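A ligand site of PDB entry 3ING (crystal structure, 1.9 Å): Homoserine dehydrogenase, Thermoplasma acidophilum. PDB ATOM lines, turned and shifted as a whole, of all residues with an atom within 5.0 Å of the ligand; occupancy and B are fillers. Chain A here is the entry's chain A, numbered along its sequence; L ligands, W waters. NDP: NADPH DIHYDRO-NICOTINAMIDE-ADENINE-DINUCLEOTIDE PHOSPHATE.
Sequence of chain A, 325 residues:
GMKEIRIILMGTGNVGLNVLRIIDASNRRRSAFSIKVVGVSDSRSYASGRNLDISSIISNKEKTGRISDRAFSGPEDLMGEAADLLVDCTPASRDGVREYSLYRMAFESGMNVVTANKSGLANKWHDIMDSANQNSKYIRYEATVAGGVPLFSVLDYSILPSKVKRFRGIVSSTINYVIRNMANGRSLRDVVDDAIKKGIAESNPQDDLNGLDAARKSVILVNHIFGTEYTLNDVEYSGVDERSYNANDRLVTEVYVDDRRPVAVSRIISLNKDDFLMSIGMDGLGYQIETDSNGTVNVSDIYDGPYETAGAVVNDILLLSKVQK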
ATOM      1  N   MET A  10      -0.410  13.374  14.128  1.00  0.00           N
ATOM      2  CA  MET A  10      -1.106  12.332  14.833  1.00  0.00           C
ATOM      3  C   MET A  10      -1.134  12.716  16.318  1.00  0.00           C
ATOM      4  O   MET A  10      -0.082  12.770  16.938  1.00  0.00           O
ATOM      5  CB  MET A  10      -0.362  11.017  14.707  1.00  0.00           C
ATOM      6  CG  MET A  10      -0.220  10.439  13.331  1.00  0.00           C
ATOM      7  SD  MET A  10      -1.698   9.302  12.896  1.00  0.00           S
ATOM      8  CE  MET A  10      -1.749   7.958  14.274  1.00  0.00           C
ATOM      9  N   GLY A  11      -2.318  12.974  16.869  1.00  0.00           N
ATOM     10  CA  GLY A  11      -2.457  13.360  18.270  1.00  0.00           C
ATOM     11  C   GLY A  11      -2.564  14.850  18.421  1.00  0.00           C
ATOM     12  O   GLY A  11      -1.691  15.588  17.977  1.00  0.00           O
ATOM     13  N   THR A  12      -3.669  15.288  19.020  1.00  0.00           N
ATOM     14  CA  THR A  12      -4.006  16.702  19.203  1.00  0.00           C
ATOM     15  C   THR A  12      -4.472  16.984  20.641  1.00  0.00           C
ATOM     16  O   THR A  12      -5.523  17.641  20.885  1.00  0.00           O
ATOM     17  CB  THR A  12      -5.075  17.128  18.228  1.00  0.00           C
ATOM     18  OG1 THR A  12      -6.038  16.084  18.117  1.00  0.00           O
ATOM     19  CG2 THR A  12      -4.454  17.373  16.847  1.00  0.00           C
ATOM     20  N   GLY A  13      -3.660  16.501  21.582  1.00  0.00           N
ATOM     21  CA  GLY A  13      -3.901  16.720  23.004  1.00  0.00           C
ATOM     22  C   GLY A  13      -3.134  17.937  23.498  1.00  0.00           C
ATOM     23  O   GLY A  13      -2.985  18.912  22.760  1.00  0.00           O
ATOM     24  N   ASN A  14      -2.643  17.887  24.723  1.00  0.00           N
ATOM     25  CA  ASN A  14      -1.904  19.003  25.317  1.00  0.00           C
ATOM     26  C   ASN A  14      -0.810  19.505  24.390  1.00  0.00           C
ATOM     27  O   ASN A  14      -0.658  20.706  24.159  1.00  0.00           O
ATOM     28  CB  ASN A  14      -1.260  18.581  26.642  1.00  0.00           C
ATOM     29  CG  ASN A  14      -2.275  18.339  27.724  1.00  0.00           C
ATOM     30  OD1 ASN A  14      -3.446  18.551  27.511  1.00  0.00           O
ATOM     31  ND2 ASN A  14      -1.843  17.858  28.875  1.00  0.00           N
ATOM     32  N   VAL A  15      -0.053  18.581  23.847  1.00  0.00           N
ATOM     33  CA  VAL A  15       1.084  18.976  23.022  1.00  0.00           C
ATOM     34  C   VAL A  15       0.650  19.222  21.569  1.00  0.00           C
ATOM     35  O   VAL A  15       0.943  20.255  21.014  1.00  0.00           O
ATOM     36  CB  VAL A  15       2.235  17.906  23.059  1.00  0.00           C
ATOM     37  CG1 VAL A  15       3.303  18.248  22.040  1.00  0.00           C
ATOM     38  CG2 VAL A  15       2.849  17.764  24.474  1.00  0.00           C
ATOM     39  N   GLY A  16      -0.051  18.265  20.966  1.00  0.00           N
ATOM     40  CA  GLY A  16      -0.486  18.398  19.585  1.00  0.00           C
ATOM     41  C   GLY A  16      -1.385  19.590  19.274  1.00  0.00           C
ATOM     42  O   GLY A  16      -1.218  20.227  18.232  1.00  0.00           O
ATOM     43  N   SER A  41      -5.167  14.007  13.323  1.00  0.00           N
ATOM     44  CA  SER A  41      -6.026  13.115  14.131  1.00  0.00           C
ATOM     45  C   SER A  41      -6.014  13.290  15.685  1.00  0.00           C
ATOM     46  O   SER A  41      -5.157  13.883  16.235  1.00  0.00           O
ATOM     47  CB  SER A  41      -5.661  11.655  13.866  1.00  0.00           C
ATOM     48  OG  SER A  41      -4.278  11.403  14.170  1.00  0.00           O
ATOM     49  N   ASP A  42      -7.092  12.753  16.323  1.00  0.00           N
ATOM     50  CA  ASP A  42      -7.138  12.434  17.704  1.00  0.00           C
ATOM     51  C   ASP A  42      -7.560  10.942  17.742  1.00  0.00           C
ATOM     52  O   ASP A  42      -7.518  10.272  16.727  1.00  0.00           O
ATOM     53  CB  ASP A  42      -8.066  13.357  18.500  1.00  0.00           C
ATOM     54  CG  ASP A  42      -9.513  13.325  18.055  1.00  0.00           C
ATOM     55  OD1 ASP A  42     -10.019  12.294  17.529  1.00  0.00           O
ATOM     56  OD2 ASP A  42     -10.179  14.332  18.340  1.00  0.00           O
ATOM     57  N   SER A  43      -7.929  10.424  18.902  1.00  0.00           N
ATOM     58  CA  SER A  43      -8.156   8.982  19.004  1.00  0.00           C
ATOM     59  C   SER A  43      -9.395   8.534  18.261  1.00  0.00           C
ATOM     60  O   SER A  43      -9.484   7.367  17.876  1.00  0.00           O
ATOM     61  CB  SER A  43      -8.274   8.559  20.475  1.00  0.00           C
ATOM     62  OG  SER A  43      -9.357   9.212  21.096  1.00  0.00           O
ATOM     63  N   ARG A  44     -10.337   9.445  18.063  1.00  0.00           N
ATOM     64  CA  ARG A  44     -11.611   9.083  17.446  1.00  0.00           C
ATOM     65  C   ARG A  44     -11.914   9.627  16.071  1.00  0.00           C
ATOM     66  O   ARG A  44     -12.727   9.053  15.376  1.00  0.00           O
ATOM     67  CB  ARG A  44     -12.724   9.588  18.359  1.00  0.00           C
ATOM     68  CG  ARG A  44     -12.753   8.939  19.720  1.00  0.00           C
ATOM     69  CD  ARG A  44     -13.888   9.532  20.545  1.00  0.00           C
ATOM     70  NE  ARG A  44     -13.573  10.869  21.042  1.00  0.00           N
ATOM     71  CZ  ARG A  44     -14.462  11.735  21.545  1.00  0.00           C
ATOM     72  NH1 ARG A  44     -15.753  11.421  21.661  1.00  0.00           N
ATOM     73  NH2 ARG A  44     -14.052  12.926  21.969  1.00  0.00           N
ATOM     74  N   LYS A  61     -11.846  21.369  18.068  1.00  0.00           N
ATOM     75  CA  LYS A  61     -11.297  20.504  19.108  1.00  0.00           C
ATOM     76  C   LYS A  61     -11.506  21.085  20.514  1.00  0.00           C
ATOM     77  O   LYS A  61     -11.925  20.386  21.423  1.00  0.00           O
ATOM     78  CB  LYS A  61      -9.811  20.306  18.845  1.00  0.00           C
ATOM     79  CG  LYS A  61      -9.066  19.332  19.775  1.00  0.00           C
ATOM     80  CD  LYS A  61      -9.729  17.928  19.824  1.00  0.00           C
ATOM     81  CE  LYS A  61      -8.885  16.983  20.618  1.00  0.00           C
ATOM     82  NZ  LYS A  61      -9.508  15.599  20.716  1.00  0.00           N
ATOM     83  N   GLY A  65     -14.215  18.776  21.790  1.00  0.00           N
ATOM     84  CA  GLY A  65     -13.364  17.670  22.206  1.00  0.00           C
ATOM     85  C   GLY A  65     -12.998  16.720  21.084  1.00  0.00           C
ATOM     86  O   GLY A  65     -12.347  15.700  21.320  1.00  0.00           O
ATOM     87  N   PHE A  72     -11.899   7.948  12.762  1.00  0.00           N
ATOM     88  CA  PHE A  72     -10.524   7.573  12.499  1.00  0.00           C
ATOM     89  C   PHE A  72     -10.254   6.116  12.832  1.00  0.00           C
ATOM     90  O   PHE A  72     -10.466   5.704  13.964  1.00  0.00           O
ATOM     91  CB  PHE A  72      -9.619   8.448  13.353  1.00  0.00           C
ATOM     92  CG  PHE A  72      -8.133   8.213  13.136  1.00  0.00           C
ATOM     93  CD1 PHE A  72      -7.541   8.521  11.926  1.00  0.00           C
ATOM     94  CD2 PHE A  72      -7.330   7.743  14.167  1.00  0.00           C
ATOM     95  CE1 PHE A  72      -6.197   8.363  11.734  1.00  0.00           C
ATOM     96  CE2 PHE A  72      -5.972   7.581  13.976  1.00  0.00           C
ATOM     97  CZ  PHE A  72      -5.417   7.891  12.765  1.00  0.00           C
ATOM     98  N   CYS A  89       2.417  13.007  18.129  1.00  0.00           N
ATOM     99  CA  CYS A  89       2.120  13.520  19.435  1.00  0.00           C
ATOM    100  C   CYS A  89       1.106  12.607  20.164  1.00  0.00           C
ATOM    101  O   CYS A  89       0.254  13.070  20.944  1.00  0.00           O
ATOM    102  CB  CYS A  89       1.570  14.943  19.319  1.00  0.00           C
ATOM    103  SG  CYS A  89       2.837  16.141  18.794  1.00  0.00           S
ATOM    104  N   THR A  90       1.164  11.329  19.862  1.00  0.00           N
ATOM    105  CA  THR A  90       0.269  10.327  20.506  1.00  0.00           C
ATOM    106  C   THR A  90       0.918   9.871  21.818  1.00  0.00           C
ATOM    107  O   THR A  90       2.096  10.066  22.017  1.00  0.00           O
ATOM    108  CB  THR A  90       0.054   9.097  19.613  1.00  0.00           C
ATOM    109  OG1 THR A  90       1.298   8.416  19.467  1.00  0.00           O
ATOM    110  CG2 THR A  90      -0.498   9.490  18.233  1.00  0.00           C
ATOM    111  N   PRO A  91       0.128   9.295  22.750  1.00  0.00           N
ATOM    112  CA  PRO A  91       0.684   8.811  24.005  1.00  0.00           C
ATOM    113  C   PRO A  91       1.528   7.578  23.835  1.00  0.00           C
ATOM    114  O   PRO A  91       1.384   6.833  22.842  1.00  0.00           O
ATOM    115  CB  PRO A  91      -0.581   8.460  24.820  1.00  0.00           C
ATOM    116  CG  PRO A  91      -1.735   8.976  24.083  1.00  0.00           C
ATOM    117  CD  PRO A  91      -1.313   9.059  22.678  1.00  0.00           C
ATOM    118  N   ALA A  92       2.385   7.314  24.817  1.00  0.00           N
ATOM    119  CA  ALA A  92       3.209   6.130  24.841  1.00  0.00           C
ATOM    120  C   ALA A  92       2.407   4.858  24.896  1.00  0.00           C
ATOM    121  O   ALA A  92       1.524   4.709  25.718  1.00  0.00           O
ATOM    122  CB  ALA A  92       4.174   6.188  26.040  1.00  0.00           C
ATOM    123  N   ARG A  98       3.365   0.033  18.150  1.00  0.00           N
ATOM    124  CA  ARG A  98       2.470   0.916  17.419  1.00  0.00           C
ATOM    125  C   ARG A  98       3.242   2.077  16.754  1.00  0.00           C
ATOM    126  O   ARG A  98       3.022   2.416  15.580  1.00  0.00           O
ATOM    127  CB  ARG A  98       1.377   1.451  18.367  1.00  0.00           C
ATOM    128  CG  ARG A  98       0.374   2.346  17.652  1.00  0.00           C
ATOM    129  CD  ARG A  98      -0.725   2.929  18.561  1.00  0.00           C
ATOM    130  NE  ARG A  98      -0.181   3.749  19.635  1.00  0.00           N
ATOM    131  CZ  ARG A  98       0.327   4.976  19.473  1.00  0.00           C
ATOM    132  NH1 ARG A  98       0.407   5.559  18.278  1.00  0.00           N
ATOM    133  NH2 ARG A  98       0.792   5.620  20.518  1.00  0.00           N
ATOM    134  N   ALA A 116       7.343  13.513  19.549  1.00  0.00           N
ATOM    135  CA  ALA A 116       7.341  13.823  20.997  1.00  0.00           C
ATOM    136  C   ALA A 116       7.135  12.569  21.837  1.00  0.00           C
ATOM    137  O   ALA A 116       7.369  12.571  23.049  1.00  0.00           O
ATOM    138  CB  ALA A 116       6.160  14.839  21.316  1.00  0.00           C
ATOM    139  N   ASN A 117       6.667  11.513  21.194  1.00  0.00           N
ATOM    140  CA  ASN A 117       6.373  10.245  21.853  1.00  0.00           C
ATOM    141  C   ASN A 117       7.695   9.479  22.069  1.00  0.00           C
ATOM    142  O   ASN A 117       8.469   9.326  21.138  1.00  0.00           O
ATOM    143  CB  ASN A 117       5.334   9.496  21.015  1.00  0.00           C
ATOM    144  CG  ASN A 117       5.070   8.059  21.492  1.00  0.00           C
ATOM    145  OD1 ASN A 117       5.966   7.401  21.938  1.00  0.00           O
ATOM    146  ND2 ASN A 117       3.844   7.578  21.335  1.00  0.00           N
ATOM    147  N   LYS A 118       7.941   9.040  23.312  1.00  0.00           N
ATOM    148  CA  LYS A 118       9.185   8.406  23.716  1.00  0.00           C
ATOM    149  C   LYS A 118       9.203   6.899  23.609  1.00  0.00           C
ATOM    150  O   LYS A 118      10.268   6.288  23.681  1.00  0.00           O
ATOM    151  CB  LYS A 118       9.454   8.767  25.188  1.00  0.00           C
ATOM    152  CG  LYS A 118       9.437  10.265  25.368  1.00  0.00           C
ATOM    153  CD  LYS A 118       9.165  10.708  26.778  1.00  0.00           C
ATOM    154  CE  LYS A 118       8.548  12.125  26.764  1.00  0.00           C
ATOM    155  NZ  LYS A 118       8.147  12.568  28.132  1.00  0.00           N
ATOM    156  N   ALA A 143      11.468  16.834  21.456  1.00  0.00           N
ATOM    157  CA  ALA A 143      10.485  16.829  22.536  1.00  0.00           C
ATOM    158  C   ALA A 143      10.467  15.593  23.405  1.00  0.00           C
ATOM    159  O   ALA A 143       9.846  15.609  24.454  1.00  0.00           O
ATOM    160  CB  ALA A 143       9.068  17.073  21.927  1.00  0.00           C
ATOM    161  N   THR A 144      11.131  14.503  22.993  1.00  0.00           N
ATOM    162  CA  THR A 144      11.118  13.260  23.752  1.00  0.00           C
ATOM    163  C   THR A 144      11.963  13.302  25.034  1.00  0.00           C
ATOM    164  O   THR A 144      11.732  12.499  25.882  1.00  0.00           O
ATOM    165  CB  THR A 144      11.600  12.059  22.921  1.00  0.00           C
ATOM    166  OG1 THR A 144      13.008  12.248  22.605  1.00  0.00           O
ATOM    167  CG2 THR A 144      10.737  11.904  21.650  1.00  0.00           C
ATOM    168  N   GLY A 147      11.025  18.036  27.413  1.00  0.00           N
ATOM    169  CA  GLY A 147      10.096  18.773  26.566  1.00  0.00           C
ATOM    170  C   GLY A 147      10.624  19.997  25.846  1.00  0.00           C
ATOM    171  O   GLY A 147      11.127  19.915  24.737  1.00  0.00           O
ATOM    172  N   GLY A 199      -0.405  20.375  32.583  1.00  0.00           N
ATOM    173  CA  GLY A 199      -0.383  19.637  31.327  1.00  0.00           C
ATOM    174  C   GLY A 199       0.845  18.788  31.140  1.00  0.00           C
ATOM    175  O   GLY A 199       1.054  18.320  30.018  1.00  0.00           O
ATOM    176  N   ILE A 200       1.599  18.542  32.210  1.00  0.00           N
ATOM    177  CA  ILE A 200       2.861  17.816  32.143  1.00  0.00           C
ATOM    178  C   ILE A 200       2.743  16.314  32.461  1.00  0.00           C
ATOM    179  O   ILE A 200       3.675  15.599  32.195  1.00  0.00           O
ATOM    180  CB  ILE A 200       3.968  18.416  33.091  1.00  0.00           C
ATOM    181  CG1 ILE A 200       3.551  18.335  34.556  1.00  0.00           C
ATOM    182  CG2 ILE A 200       4.366  19.889  32.659  1.00  0.00           C
ATOM    183  CD1 ILE A 200       4.672  18.659  35.656  1.00  0.00           C
ATOM    184  N   ALA A 201       1.658  15.845  33.045  1.00  0.00           N
ATOM    185  CA  ALA A 201       1.527  14.437  33.406  1.00  0.00           C
ATOM    186  C   ALA A 201       1.321  13.599  32.166  1.00  0.00           C
ATOM    187  O   ALA A 201       0.658  14.036  31.224  1.00  0.00           O
ATOM    188  CB  ALA A 201       0.341  14.255  34.334  1.00  0.00           C
ATOM    189  N   GLU A 202       1.846  12.373  32.175  1.00  0.00           N
ATOM    190  CA  GLU A 202       1.669  11.442  31.094  1.00  0.00           C
ATOM    191  C   GLU A 202       0.232  10.992  31.041  1.00  0.00           C
ATOM    192  O   GLU A 202      -0.459  10.963  32.057  1.00  0.00           O
ATOM    193  CB  GLU A 202       2.557  10.217  31.330  1.00  0.00           C
ATOM    194  CG  GLU A 202       4.020  10.480  31.051  1.00  0.00           C
ATOM    195  CD  GLU A 202       4.297  10.481  29.579  1.00  0.00           C
ATOM    196  OE1 GLU A 202       4.497   9.382  29.012  1.00  0.00           O
ATOM    197  OE2 GLU A 202       4.288  11.584  28.999  1.00  0.00           O
ATOM    198  N   SER A 203      -0.206  10.611  29.836  1.00  0.00           N
ATOM    199  CA  SER A 203      -1.528  10.080  29.576  1.00  0.00           C
ATOM    200  C   SER A 203      -1.822   8.899  30.503  1.00  0.00           C
ATOM    201  O   SER A 203      -2.989   8.626  30.837  1.00  0.00           O
ATOM    202  CB  SER A 203      -1.652   9.682  28.092  1.00  0.00           C
ATOM    203  OG  SER A 203      -1.388  10.811  27.276  1.00  0.00           O
ATOM    204  N   ASP A 213       8.821   7.080  32.613  1.00  0.00           N
ATOM    205  CA  ASP A 213       9.039   8.238  31.719  1.00  0.00           C
ATOM    206  C   ASP A 213      10.526   8.567  31.724  1.00  0.00           C
ATOM    207  O   ASP A 213      11.122   8.745  30.670  1.00  0.00           O
ATOM    208  CB  ASP A 213       8.205   9.437  32.170  1.00  0.00           C
ATOM    209  CG  ASP A 213       8.455  10.691  31.320  1.00  0.00           C
ATOM    210  OD1 ASP A 213       8.059  10.723  30.151  1.00  0.00           O
ATOM    211  OD2 ASP A 213       9.029  11.679  31.845  1.00  0.00           O
ATOM    212  N   LYS A 217      13.427   8.190  28.517  1.00  0.00           N
ATOM    213  CA  LYS A 217      14.286   9.301  28.126  1.00  0.00           C
ATOM    214  C   LYS A 217      15.739   8.860  28.202  1.00  0.00           C
ATOM    215  O   LYS A 217      16.524   9.231  27.368  1.00  0.00           O
ATOM    216  CB  LYS A 217      14.030  10.535  29.014  1.00  0.00           C
ATOM    217  CG  LYS A 217      12.636  11.094  28.897  1.00  0.00           C
ATOM    218  CD  LYS A 217      12.443  12.321  29.807  1.00  0.00           C
ATOM    219  CE  LYS A 217      11.017  12.887  29.637  1.00  0.00           C
ATOM    220  NZ  LYS A 217      10.781  13.552  28.342  1.00  0.00           N
ATOM    221  N   GLY A 305       6.304  23.278  29.803  1.00  0.00           N
ATOM    222  CA  GLY A 305       4.939  22.807  29.674  1.00  0.00           C
ATOM    223  C   GLY A 305       4.703  22.296  28.291  1.00  0.00           C
ATOM    224  O   GLY A 305       5.632  22.298  27.476  1.00  0.00           O
ATOM    225  N   PRO A 306       3.472  21.848  28.016  1.00  0.00           N
ATOM    226  CA  PRO A 306       3.128  21.334  26.684  1.00  0.00           C
ATOM    227  C   PRO A 306       3.248  22.382  25.566  1.00  0.00           C
ATOM    228  O   PRO A 306       3.480  22.016  24.426  1.00  0.00           O
ATOM    229  CB  PRO A 306       1.696  20.847  26.852  1.00  0.00           C
ATOM    230  CG  PRO A 306       1.182  21.575  28.034  1.00  0.00           C
ATOM    231  CD  PRO A 306       2.335  21.785  28.932  1.00  0.00           C
ATOM    232  N   THR A 309       6.984  22.346  24.816  1.00  0.00           N
ATOM    233  CA  THR A 309       7.253  21.083  24.157  1.00  0.00           C
ATOM    234  C   THR A 309       6.806  21.183  22.700  1.00  0.00           C
ATOM    235  O   THR A 309       7.528  20.753  21.811  1.00  0.00           O
ATOM    236  CB  THR A 309       6.480  19.956  24.887  1.00  0.00           C
ATOM    237  OG1 THR A 309       6.923  19.848  26.254  1.00  0.00           O
ATOM    238  CG2 THR A 309       6.610  18.562  24.191  1.00  0.00           C
HETATM  239  PA  NDP L   1      -2.591  13.736  25.502  1.00  0.00           P
HETATM  240  O1A NDP L   1      -3.022  15.047  26.028  1.00  0.00           O
HETATM  241  O2A NDP L   1      -3.160  12.535  26.156  1.00  0.00           O
HETATM  242  O5B NDP L   1      -2.936  13.628  23.932  1.00  0.00           O
HETATM  243  C5B NDP L   1      -2.765  12.481  23.139  1.00  0.00           C
HETATM  244  C4B NDP L   1      -3.426  12.679  21.784  1.00  0.00           C
HETATM  245  O4B NDP L   1      -3.366  11.508  21.004  1.00  0.00           O
HETATM  246  C3B NDP L   1      -4.927  12.947  21.913  1.00  0.00           C
HETATM  247  O3B NDP L   1      -5.413  13.682  20.795  1.00  0.00           O
HETATM  248  C2B NDP L   1      -5.519  11.572  21.907  1.00  0.00           C
HETATM  249  O2B NDP L   1      -6.859  11.516  21.508  1.00  0.00           O
HETATM  250  C1B NDP L   1      -4.665  10.949  20.831  1.00  0.00           C
HETATM  251  N9A NDP L   1      -4.561   9.500  20.897  1.00  0.00           N
HETATM  252  C8A NDP L   1      -4.603   8.635  21.961  1.00  0.00           C
HETATM  253  N7A NDP L   1      -4.383   7.365  21.476  1.00  0.00           N
HETATM  254  C5A NDP L   1      -4.217   7.449  20.151  1.00  0.00           C
HETATM  255  C6A NDP L   1      -3.993   6.456  19.218  1.00  0.00           C
HETATM  256  N6A NDP L   1      -3.608   5.235  19.600  1.00  0.00           N
HETATM  257  N1A NDP L   1      -3.862   6.866  17.943  1.00  0.00           N
HETATM  258  C2A NDP L   1      -3.982   8.185  17.545  1.00  0.00           C
HETATM  259  N3A NDP L   1      -4.193   9.194  18.465  1.00  0.00           N
HETATM  260  C4A NDP L   1      -4.306   8.773  19.752  1.00  0.00           C
HETATM  261  O3  NDP L   1      -0.990  13.647  25.534  1.00  0.00           O
HETATM  262  PN  NDP L   1       0.042  14.882  25.529  1.00  0.00           P
HETATM  263  O1N NDP L   1       0.147  15.427  26.924  1.00  0.00           O
HETATM  264  O2N NDP L   1      -0.347  15.774  24.404  1.00  0.00           O
HETATM  265  O5D NDP L   1       1.462  14.161  25.209  1.00  0.00           O
HETATM  266  C5D NDP L   1       1.597  13.667  23.867  1.00  0.00           C
HETATM  267  C4D NDP L   1       2.965  13.008  23.718  1.00  0.00           C
HETATM  268  O4D NDP L   1       3.943  13.986  23.984  1.00  0.00           O
HETATM  269  C3D NDP L   1       3.219  11.899  24.709  1.00  0.00           C
HETATM  270  O3D NDP L   1       3.824  10.742  24.115  1.00  0.00           O
HETATM  271  C2D NDP L   1       4.109  12.537  25.759  1.00  0.00           C
HETATM  272  O2D NDP L   1       4.939  11.616  26.416  1.00  0.00           O
HETATM  273  C1D NDP L   1       4.893  13.522  24.923  1.00  0.00           C
HETATM  274  N1N NDP L   1       5.481  14.611  25.694  1.00  0.00           N
HETATM  275  C2N NDP L   1       4.665  15.402  26.445  1.00  0.00           C
HETATM  276  C3N NDP L   1       5.173  16.344  27.343  1.00  0.00           C
HETATM  277  C7N NDP L   1       4.241  17.275  28.016  1.00  0.00           C
HETATM  278  O7N NDP L   1       4.702  18.548  28.232  1.00  0.00           O
HETATM  279  N7N NDP L   1       2.981  16.949  28.277  1.00  0.00           N
HETATM  280  C4N NDP L   1       6.634  16.771  27.268  1.00  0.00           C
HETATM  281  C5N NDP L   1       7.423  15.857  26.377  1.00  0.00           C
HETATM  282  C6N NDP L   1       6.828  14.850  25.632  1.00  0.00           C
HETATM  283  P2B NDP L   1      -8.017  12.384  22.200  1.00  0.00           P
HETATM  284  O1X NDP L   1      -9.226  11.750  21.553  1.00  0.00           O
HETATM  285  O2X NDP L   1      -7.810  13.915  22.020  1.00  0.00           O
HETATM  286  O3X NDP L   1      -7.910  12.046  23.647  1.00  0.00           O
HETATM  287  O   HOH W   1       1.236  11.571  27.435  1.00  0.00           O
HETATM  288  O   HOH W   2       2.688   9.184  27.108  1.00  0.00           O
HETATM  289  O   HOH W   3      -0.948  15.558  21.743  1.00  0.00           O
HETATM  290  O   HOH W   4       1.909  14.062  28.435  1.00  0.00           O
HETATM  291  O   HOH W   5       5.896   9.212  25.436  1.00  0.00           O
HETATM  292  O   HOH W   6     -11.551  12.604  20.467  1.00  0.00           O
HETATM  293  O   HOH W   7      -7.494  16.057  23.936  1.00  0.00           O
HETATM  294  O   HOH W   8       6.112  13.647  29.082  1.00  0.00           O
HETATM  295  O   HOH W   9      -4.815  10.201  25.321  1.00  0.00           O
HETATM  296  O   HOH W  10      -3.110   5.126  15.872  1.00  0.00           O
HETATM  297  O   HOH W  11      -7.587   9.823  24.672  1.00  0.00           O
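The side-chain amino group (NZ) of Lys 61 lies within salt-bridge range of the side-chain carboxylate (OD2) of Asp 42 (2.8 Å).
The side-chain amide nitrogen (ND2) of Asn 117 sits at hydrogen-bond distance from the backbone carbonyl oxygen (O) of Thr 90 (3.1 Å).
The side-chain hydroxyl (OG1) of Thr 90 sits at hydrogen-bond distance from the guanidinium group (NH2) of Arg 98, 3.0 Å away.
The backbone NH (N) of Thr 90 lies within hydrogen-bond range of the backbone carbonyl oxygen (O) of Met 10.
The side-chain amide nitrogen (ND2) of Asn 14 is in hydrogen-bond range of the backbone carbonyl oxygen (O) of Gly 199 (3.1 Å).
OG1 of Thr 309 sits at hydrogen-bond distance from O of Gly 305 (3.0 Å).
The backbone carbonyl oxygen of Met 10 is in hydrogen-bond range of the backbone NH of Cys 89 (2.8 Å).
The side-chain carboxylate (OD1) of Asp 42 lies within hydrogen-bond range of the backbone NH (N) of Arg 44 (2.9 Å).
Water W4 lies within hydrogen-bond range of O1N of the ligand (2.7 Å), O of Ala 201 (3.1 Å) and OE2 of Glu 202 (3.5 Å).
Water W6 lies within hydrogen-bond range of an oxygen (O1X) of the ligand (2.7 Å), the guanidinium group (NE) of Arg 44 (2.7 Å), the side-chain carboxylate (OD2) of Asp 42 (3.1 Å) and the backbone carbonyl oxygen (O) of Gly 65 (3.3 Å).
Water W3 lies within hydrogen-bond range of an oxygen (O2N) of the ligand (2.7 Å), the backbone NH of Gly 13 (2.9 Å), the backbone carbonyl oxygen of Cys 89 (2.9 Å) and the backbone NH of Gly 16 (3.0 Å).
Water W8 lies within hydrogen-bond range of the side-chain amino group (NZ) of Lys 118 (2.5 Å) and the side-chain carboxylate (OE2) of Glu 202 (2.8 Å).
Water W2 lies within hydrogen-bond range of OE1 of Glu 202 (2.6 Å), N of Ala 92 (3.0 Å) and O2D of the ligand (3.4 Å).
Water W1 lies within hydrogen-bond range of OG of Ser 203 (2.7 Å), O5D of the ligand (3.4 Å) and OE2 of Glu 202 (3.4 Å).
N of Ser 43 lies within hydrogen-bond range of O2B of the ligand, 3.0 Å away.
An oxygen (O1X) of the ligand is in hydrogen-bond range of the side-chain hydroxyl of Ser 43 (2.6 Å).
An oxygen (O2D) of the ligand sits at hydrogen-bond distance from the side-chain carboxylate (OE2) of Glu 202, at 2.7 Å.
OG of Ser 203 is in hydrogen-bond range of O2A of the ligand, 2.7 Å away.
O2X of the ligand lies within salt-bridge range of NZ of Lys 61 (2.7 Å).
The backbone carbonyl oxygen (O) of Thr 90 is in hydrogen-bond range of an oxygen (O3D) of the ligand (2.8 Å).
The backbone NH of Val 15 sits at hydrogen-bond distance from an oxygen (O2N) of the ligand (2.9 Å).
O of Gly 199 is in hydrogen-bond range of N7N of the ligand (2.9 Å).
An oxygen (O3B) of the ligand sits at hydrogen-bond distance from the backbone NH of Thr 12.
O2N of the ligand is in hydrogen-bond range of N of Asn 14.
The side-chain hydroxyl (OG1) of Thr 309 lies within hydrogen-bond range of an oxygen (O7N) of the ligand, at 3.2 Å.
O3B of the ligand is in hydrogen-bond range of N of Gly 13 (3.4 Å).
Merely in contact with the ligand: Ala 143 (3.1 Å), Ala 116 (3.2 Å), Cys 89 (3.3 Å), Pro 91 (3.4 Å), Lys 118 (3.4 Å), Gly 11 (3.4 Å), Asn 117 (3.4 Å), Asp 42 (3.5 Å), Pro 306 (3.5 Å), Arg 98 (3.7 Å), Gly 305 (3.7 Å), Ala 92 (3.8 Å), Gly 147 (3.96 Å), Ile 200 (3.96 Å) and Met 10 (3.97 Å).
Hydrophobic or aromatic side chains that line the ligand: Met 10, Val 15, Pro 91 and Ala 116.
Of the 35 residues printed, 26 come within 4 Å of the ligand.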
